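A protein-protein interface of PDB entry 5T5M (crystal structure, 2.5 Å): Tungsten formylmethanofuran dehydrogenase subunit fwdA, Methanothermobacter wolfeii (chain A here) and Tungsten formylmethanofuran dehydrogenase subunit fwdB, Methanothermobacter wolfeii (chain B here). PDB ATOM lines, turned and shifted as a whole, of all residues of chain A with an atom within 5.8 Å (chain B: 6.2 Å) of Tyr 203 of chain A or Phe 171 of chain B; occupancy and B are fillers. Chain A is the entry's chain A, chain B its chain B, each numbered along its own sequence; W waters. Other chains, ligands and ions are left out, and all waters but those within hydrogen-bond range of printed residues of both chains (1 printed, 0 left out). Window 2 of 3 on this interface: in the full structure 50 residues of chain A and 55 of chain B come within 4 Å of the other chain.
Tyr 203 of chain A touches two residues of chain B.
Phe 171 of chain B touches three residues of chain A.
Of the printed residues of chain A, Phe 170 of chain B touches Tyr 203 (3.4 Å).
Printed residues of chain A within 4 Å of Arg 172 of chain B: Trp 190 (3.9 Å).
Printed residues of chain B within 4 Å of Trp 190 of chain A: Arg 142, Phe 171, Arg 172 and Gln 246.
Of the printed residues of chain A, Arg 142 of chain B touches Trp 147 (3.6 Å), Glu 186 (3.0 Å) and Trp 190 (3.4 Å).
Of the printed residues of chain A, Gln 246 of chain B touches Trp 190 (3.6 Å).
Pro 202 of chain A touches none of the printed residues of chain B.
Asp 205 of chain A touches none of the printed residues of chain B.
The nearest printed residue of chain B that does not touch Tyr 203 of chain A is Arg 142 of chain B (7.9 Å).
The nearest printed residue of chain A that does not touch Gln 246 of chain B is Pro 202 of chain A (9.3 Å).
The side-chain carboxylate (OE1) of Glu 186 of chain A is in salt-bridge range of the guanidinium group (NH1) of Arg 142 of chain B, at 3.0 Å.
NH2 of Arg 142 of chain B lies close to NE1 of Trp 190 of chain A.
NE1 of Trp 147 of chain A sits at hydrogen-bond distance from OE1 of Glu 186 of chain A, 2.8 Å away.
N of Phe 170 of chain B lies within hydrogen-bond range of OD1 of Asn 141 of chain B (2.8 Å).
The backbone carbonyl oxygen (O) of Asn 141 of chain B sits at hydrogen-bond distance from the backbone NH (N) of Phe 171 of chain B (3.0 Å).
O of Arg 142 of chain B lies within hydrogen-bond range of NE of Arg 172 of chain B (2.8 Å).
OE1 of Gln 246 of chain B lies within hydrogen-bond range of NH2 of Arg 172 of chain B (2.9 Å).
Among the printed residues, merely in contact across the chains: Tyr 203 of chain A with Phe 170 of chain B, Trp 190 of chain A with Phe 171 of chain B, Trp 147 of chain A with Arg 142 of chain B, Trp 190 of chain A with Gln 246 of chain B, Trp 147 of chain A with Phe 171 of chain B, Trp 190 of chain A with Arg 172 of chain B and Tyr 203 of chain A with Phe 171 of chain B.
Water W1 bridges O of Gln 246 of chain B and O of Trp 190 of chain A.
Hydrophobic or aromatic side chains of chain A that line the printed part of chain B: Trp 147, Trp 190 and Tyr 203.
Of the 10 printed residues of chain B, 5 touch a printed residue of chain A.
Printed residues of chain B that touch a printed residue of chain A: Arg 142, Phe 170, Phe 171, Arg 172 and Gln 246.
Hydrophobic or aromatic side chains of chain B within 4 Å of the printed part of chain A: Phe 170 and Phe 171.
Among the printed residues, 9 pairs touch across the chains.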
ATOM      1  N   TRP A 147       3.555 -35.545 -16.798  1.00  0.00           N
ATOM      2  CA  TRP A 147       3.652 -35.295 -18.239  1.00  0.00           C
ATOM      3  C   TRP A 147       2.675 -36.160 -19.030  1.00  0.00           C
ATOM      4  O   TRP A 147       2.075 -35.696 -20.005  1.00  0.00           O
ATOM      5  CB  TRP A 147       5.074 -35.547 -18.748  1.00  0.00           C
ATOM      6  CG  TRP A 147       6.055 -34.464 -18.432  1.00  0.00           C
ATOM      7  CD1 TRP A 147       5.931 -33.502 -17.479  1.00  0.00           C
ATOM      8  CD2 TRP A 147       7.324 -34.233 -19.077  1.00  0.00           C
ATOM      9  NE1 TRP A 147       7.038 -32.687 -17.486  1.00  0.00           N
ATOM     10  CE2 TRP A 147       7.907 -33.115 -18.454  1.00  0.00           C
ATOM     11  CE3 TRP A 147       8.019 -34.866 -20.118  1.00  0.00           C
ATOM     12  CZ2 TRP A 147       9.147 -32.612 -18.837  1.00  0.00           C
ATOM     13  CZ3 TRP A 147       9.251 -34.367 -20.492  1.00  0.00           C
ATOM     14  CH2 TRP A 147       9.801 -33.248 -19.858  1.00  0.00           C
ATOM     15  N   GLU A 151      -0.226 -34.583 -21.281  1.00  0.00           N
ATOM     16  CA  GLU A 151      -0.255 -34.908 -22.705  1.00  0.00           C
ATOM     17  C   GLU A 151      -1.574 -35.553 -23.095  1.00  0.00           C
ATOM     18  O   GLU A 151      -2.161 -35.208 -24.126  1.00  0.00           O
ATOM     19  CB  GLU A 151       0.909 -35.829 -23.065  1.00  0.00           C
ATOM     20  CG  GLU A 151       2.267 -35.151 -23.006  1.00  0.00           C
ATOM     21  CD  GLU A 151       2.443 -34.117 -24.096  1.00  0.00           C
ATOM     22  OE1 GLU A 151       3.083 -34.448 -25.112  1.00  0.00           O
ATOM     23  OE2 GLU A 151       1.938 -32.983 -23.944  1.00  0.00           O
ATOM     24  N   GLU A 186       5.030 -27.889 -12.803  1.00  0.00           N
ATOM     25  CA  GLU A 186       5.720 -28.071 -14.075  1.00  0.00           C
ATOM     26  C   GLU A 186       6.341 -26.760 -14.532  1.00  0.00           C
ATOM     27  O   GLU A 186       7.490 -26.738 -14.990  1.00  0.00           O
ATOM     28  CB  GLU A 186       4.751 -28.628 -15.128  1.00  0.00           C
ATOM     29  CG  GLU A 186       5.252 -28.526 -16.578  1.00  0.00           C
ATOM     30  CD  GLU A 186       6.606 -29.202 -16.812  1.00  0.00           C
ATOM     31  OE1 GLU A 186       6.912 -30.206 -16.119  1.00  0.00           O
ATOM     32  OE2 GLU A 186       7.364 -28.728 -17.698  1.00  0.00           O
ATOM     33  N   TRP A 190      11.048 -24.572 -14.803  1.00  0.00           N
ATOM     34  CA  TRP A 190      11.824 -23.499 -15.408  1.00  0.00           C
ATOM     35  C   TRP A 190      11.932 -22.285 -14.487  1.00  0.00           C
ATOM     36  O   TRP A 190      12.217 -21.175 -14.953  1.00  0.00           O
ATOM     37  CB  TRP A 190      11.201 -23.073 -16.733  1.00  0.00           C
ATOM     38  CG  TRP A 190      10.971 -24.171 -17.716  1.00  0.00           C
ATOM     39  CD1 TRP A 190       9.763 -24.698 -18.099  1.00  0.00           C
ATOM     40  CD2 TRP A 190      11.969 -24.866 -18.474  1.00  0.00           C
ATOM     41  NE1 TRP A 190       9.955 -25.682 -19.040  1.00  0.00           N
ATOM     42  CE2 TRP A 190      11.299 -25.808 -19.287  1.00  0.00           C
ATOM     43  CE3 TRP A 190      13.365 -24.788 -18.539  1.00  0.00           C
ATOM     44  CZ2 TRP A 190      11.981 -26.668 -20.152  1.00  0.00           C
ATOM     45  CZ3 TRP A 190      14.037 -25.635 -19.391  1.00  0.00           C
ATOM     46  CH2 TRP A 190      13.343 -26.567 -20.196  1.00  0.00           C
ATOM     47  N   ALA A 201       1.071 -24.092 -18.235  1.00  0.00           N
ATOM     48  CA  ALA A 201       2.521 -24.177 -18.158  1.00  0.00           C
ATOM     49  C   ALA A 201       3.139 -24.161 -19.550  1.00  0.00           C
ATOM     50  O   ALA A 201       2.463 -24.438 -20.546  1.00  0.00           O
ATOM     51  CB  ALA A 201       2.942 -25.452 -17.434  1.00  0.00           C
ATOM     52  N   PRO A 202       4.431 -23.862 -19.647  1.00  0.00           N
ATOM     53  CA  PRO A 202       5.088 -23.868 -20.961  1.00  0.00           C
ATOM     54  C   PRO A 202       4.984 -25.225 -21.645  1.00  0.00           C
ATOM     55  O   PRO A 202       4.945 -26.271 -20.995  1.00  0.00           O
ATOM     56  CB  PRO A 202       6.548 -23.517 -20.635  1.00  0.00           C
ATOM     57  CG  PRO A 202       6.499 -22.834 -19.333  1.00  0.00           C
ATOM     58  CD  PRO A 202       5.342 -23.429 -18.575  1.00  0.00           C
ATOM     59  N   TYR A 203       4.951 -25.180 -22.979  1.00  0.00           N
ATOM     60  CA  TYR A 203       4.853 -26.325 -23.889  1.00  0.00           C
ATOM     61  C   TYR A 203       3.545 -27.112 -23.798  1.00  0.00           C
ATOM     62  O   TYR A 203       2.897 -27.347 -24.823  1.00  0.00           O
ATOM     63  CB  TYR A 203       6.011 -27.309 -23.704  1.00  0.00           C
ATOM     64  CG  TYR A 203       5.818 -28.507 -24.593  1.00  0.00           C
ATOM     65  CD1 TYR A 203       6.018 -28.414 -25.964  1.00  0.00           C
ATOM     66  CD2 TYR A 203       5.375 -29.715 -24.080  1.00  0.00           C
ATOM     67  CE1 TYR A 203       5.803 -29.501 -26.793  1.00  0.00           C
ATOM     68  CE2 TYR A 203       5.163 -30.798 -24.899  1.00  0.00           C
ATOM     69  CZ  TYR A 203       5.377 -30.685 -26.253  1.00  0.00           C
ATOM     70  OH  TYR A 203       5.155 -31.776 -27.063  1.00  0.00           O
ATOM     71  N   PHE A 204       3.153 -27.549 -22.599  1.00  0.00           N
ATOM     72  CA  PHE A 204       2.036 -28.484 -22.482  1.00  0.00           C
ATOM     73  C   PHE A 204       0.683 -27.856 -22.807  1.00  0.00           C
ATOM     74  O   PHE A 204      -0.248 -28.583 -23.174  1.00  0.00           O
ATOM     75  CB  PHE A 204       2.019 -29.101 -21.084  1.00  0.00           C
ATOM     76  CG  PHE A 204       3.218 -29.953 -20.809  1.00  0.00           C
ATOM     77  CD1 PHE A 204       3.249 -31.272 -21.204  1.00  0.00           C
ATOM     78  CD2 PHE A 204       4.338 -29.419 -20.190  1.00  0.00           C
ATOM     79  CE1 PHE A 204       4.364 -32.042 -20.972  1.00  0.00           C
ATOM     80  CE2 PHE A 204       5.447 -30.193 -19.963  1.00  0.00           C
ATOM     81  CZ  PHE A 204       5.458 -31.498 -20.350  1.00  0.00           C
ATOM     82  N   ASP A 205       0.548 -26.536 -22.682  1.00  0.00           N
ATOM     83  CA  ASP A 205      -0.589 -25.814 -23.247  1.00  0.00           C
ATOM     84  C   ASP A 205      -1.920 -26.361 -22.742  1.00  0.00           C
ATOM     85  O   ASP A 205      -2.912 -26.393 -23.474  1.00  0.00           O
ATOM     86  CB  ASP A 205      -0.548 -25.857 -24.778  1.00  0.00           C
ATOM     87  CG  ASP A 205      -1.520 -24.889 -25.419  1.00  0.00           C
ATOM     88  OD1 ASP A 205      -2.040 -23.985 -24.716  1.00  0.00           O
ATOM     89  OD2 ASP A 205      -1.753 -25.037 -26.638  1.00  0.00           O
ATOM     90  N   LYS B 140      18.670 -34.255 -17.847  1.00  0.00           N
ATOM     91  CA  LYS B 140      18.679 -34.777 -19.210  1.00  0.00           C
ATOM     92  C   LYS B 140      17.738 -33.999 -20.126  1.00  0.00           C
ATOM     93  O   LYS B 140      18.095 -33.687 -21.266  1.00  0.00           O
ATOM     94  CB  LYS B 140      18.297 -36.256 -19.202  1.00  0.00           C
ATOM     95  CG  LYS B 140      18.181 -36.850 -20.592  1.00  0.00           C
ATOM     96  CD  LYS B 140      18.235 -38.369 -20.578  1.00  0.00           C
ATOM     97  CE  LYS B 140      16.872 -38.992 -20.465  1.00  0.00           C
ATOM     98  NZ  LYS B 140      16.891 -40.347 -21.072  1.00  0.00           N
ATOM     99  N   ASN B 141      16.529 -33.686 -19.654  1.00  0.00           N
ATOM    100  CA  ASN B 141      15.520 -33.101 -20.528  1.00  0.00           C
ATOM    101  C   ASN B 141      15.501 -31.575 -20.538  1.00  0.00           C
ATOM    102  O   ASN B 141      14.975 -31.000 -21.498  1.00  0.00           O
ATOM    103  CB  ASN B 141      14.131 -33.625 -20.144  1.00  0.00           C
ATOM    104  CG  ASN B 141      13.975 -35.101 -20.430  1.00  0.00           C
ATOM    105  OD1 ASN B 141      14.014 -35.521 -21.584  1.00  0.00           O
ATOM    106  ND2 ASN B 141      13.796 -35.899 -19.383  1.00  0.00           N
ATOM    107  N   ARG B 142      16.074 -30.900 -19.526  1.00  0.00           N
ATOM    108  CA  ARG B 142      15.985 -29.441 -19.417  1.00  0.00           C
ATOM    109  C   ARG B 142      17.318 -28.696 -19.435  1.00  0.00           C
ATOM    110  O   ARG B 142      17.356 -27.555 -19.906  1.00  0.00           O
ATOM    111  CB  ARG B 142      15.264 -29.040 -18.122  1.00  0.00           C
ATOM    112  CG  ARG B 142      13.843 -29.556 -17.981  1.00  0.00           C
ATOM    113  CD  ARG B 142      13.211 -29.023 -16.703  1.00  0.00           C
ATOM    114  NE  ARG B 142      12.086 -29.843 -16.254  1.00  0.00           N
ATOM    115  CZ  ARG B 142      10.809 -29.610 -16.542  1.00  0.00           C
ATOM    116  NH1 ARG B 142       9.861 -30.416 -16.076  1.00  0.00           N
ATOM    117  NH2 ARG B 142      10.470 -28.572 -17.293  1.00  0.00           N
ATOM    118  N   GLY B 169      17.562 -35.001 -24.741  1.00  0.00           N
ATOM    119  CA  GLY B 169      16.380 -34.931 -23.917  1.00  0.00           C
ATOM    120  C   GLY B 169      15.290 -34.128 -24.597  1.00  0.00           C
ATOM    121  O   GLY B 169      15.476 -33.565 -25.681  1.00  0.00           O
ATOM    122  N   PHE B 170      14.144 -34.070 -23.921  1.00  0.00           N
ATOM    123  CA  PHE B 170      12.943 -33.558 -24.571  1.00  0.00           C
ATOM    124  C   PHE B 170      13.126 -32.116 -25.032  1.00  0.00           C
ATOM    125  O   PHE B 170      12.844 -31.789 -26.187  1.00  0.00           O
ATOM    126  CB  PHE B 170      11.738 -33.677 -23.643  1.00  0.00           C
ATOM    127  CG  PHE B 170      10.449 -33.340 -24.319  1.00  0.00           C
ATOM    128  CD1 PHE B 170       9.937 -34.175 -25.302  1.00  0.00           C
ATOM    129  CD2 PHE B 170       9.768 -32.179 -24.003  1.00  0.00           C
ATOM    130  CE1 PHE B 170       8.750 -33.865 -25.953  1.00  0.00           C
ATOM    131  CE2 PHE B 170       8.587 -31.862 -24.641  1.00  0.00           C
ATOM    132  CZ  PHE B 170       8.073 -32.713 -25.627  1.00  0.00           C
ATOM    133  N   PHE B 171      13.581 -31.232 -24.139  1.00  0.00           N
ATOM    134  CA  PHE B 171      13.866 -29.847 -24.497  1.00  0.00           C
ATOM    135  C   PHE B 171      15.328 -29.628 -24.866  1.00  0.00           C
ATOM    136  O   PHE B 171      15.732 -28.481 -25.090  1.00  0.00           O
ATOM    137  CB  PHE B 171      13.483 -28.896 -23.352  1.00  0.00           C
ATOM    138  CG  PHE B 171      12.050 -29.007 -22.923  1.00  0.00           C
ATOM    139  CD1 PHE B 171      11.049 -28.355 -23.618  1.00  0.00           C
ATOM    140  CD2 PHE B 171      11.704 -29.766 -21.826  1.00  0.00           C
ATOM    141  CE1 PHE B 171       9.734 -28.468 -23.225  1.00  0.00           C
ATOM    142  CE2 PHE B 171      10.397 -29.877 -21.433  1.00  0.00           C
ATOM    143  CZ  PHE B 171       9.408 -29.229 -22.134  1.00  0.00           C
ATOM    144  N   ARG B 172      16.127 -30.698 -24.915  1.00  0.00           N
ATOM    145  CA  ARG B 172      17.542 -30.638 -25.275  1.00  0.00           C
ATOM    146  C   ARG B 172      17.842 -31.755 -26.271  1.00  0.00           C
ATOM    147  O   ARG B 172      18.645 -32.660 -26.031  1.00  0.00           O
ATOM    148  CB  ARG B 172      18.452 -30.756 -24.046  1.00  0.00           C
ATOM    149  CG  ARG B 172      18.241 -29.690 -22.981  1.00  0.00           C
ATOM    150  CD  ARG B 172      18.545 -28.288 -23.496  1.00  0.00           C
ATOM    151  NE  ARG B 172      17.999 -27.294 -22.576  1.00  0.00           N
ATOM    152  CZ  ARG B 172      17.432 -26.145 -22.935  1.00  0.00           C
ATOM    153  NH1 ARG B 172      17.323 -25.805 -24.214  1.00  0.00           N
ATOM    154  NH2 ARG B 172      16.961 -25.337 -21.995  1.00  0.00           N
ATOM    155  N   GLU B 173      17.180 -31.677 -27.423  1.00  0.00           N
ATOM    156  CA  GLU B 173      17.269 -32.766 -28.382  1.00  0.00           C
ATOM    157  C   GLU B 173      18.608 -32.818 -29.106  1.00  0.00           C
ATOM    158  O   GLU B 173      18.882 -33.818 -29.773  1.00  0.00           O
ATOM    159  CB  GLU B 173      16.112 -32.693 -29.388  1.00  0.00           C
ATOM    160  CG  GLU B 173      15.796 -31.351 -30.021  1.00  0.00           C
ATOM    161  CD  GLU B 173      14.596 -31.424 -31.010  1.00  0.00           C
ATOM    162  OE1 GLU B 173      13.944 -32.491 -31.123  1.00  0.00           O
ATOM    163  OE2 GLU B 173      14.305 -30.408 -31.680  1.00  0.00           O
ATOM    164  N   ASP B 178      23.572 -28.840 -27.081  1.00  0.00           N
ATOM    165  CA  ASP B 178      22.614 -27.941 -26.438  1.00  0.00           C
ATOM    166  C   ASP B 178      23.048 -27.501 -25.043  1.00  0.00           C
ATOM    167  O   ASP B 178      22.300 -26.780 -24.378  1.00  0.00           O
ATOM    168  CB  ASP B 178      21.223 -28.602 -26.346  1.00  0.00           C
ATOM    169  CG  ASP B 178      20.389 -28.423 -27.613  1.00  0.00           C
ATOM    170  OD1 ASP B 178      20.723 -27.556 -28.442  1.00  0.00           O
ATOM    171  OD2 ASP B 178      19.385 -29.155 -27.786  1.00  0.00           O
ATOM    172  N   GLN B 246      18.704 -21.437 -18.952  1.00  0.00           N
ATOM    173  CA  GLN B 246      17.292 -21.765 -18.789  1.00  0.00           C
ATOM    174  C   GLN B 246      17.090 -22.806 -17.708  1.00  0.00           C
ATOM    175  O   GLN B 246      16.036 -22.833 -17.068  1.00  0.00           O
ATOM    176  CB  GLN B 246      16.698 -22.269 -20.102  1.00  0.00           C
ATOM    177  CG  GLN B 246      16.827 -21.276 -21.222  1.00  0.00           C
ATOM    178  CD  GLN B 246      16.037 -21.666 -22.465  1.00  0.00           C
ATOM    179  OE1 GLN B 246      15.640 -22.817 -22.632  1.00  0.00           O
ATOM    180  NE2 GLN B 246      15.811 -20.699 -23.344  1.00  0.00           N
HETATM  181  O   HOH W   1      14.859 -20.494 -16.225  1.00  0.00           O
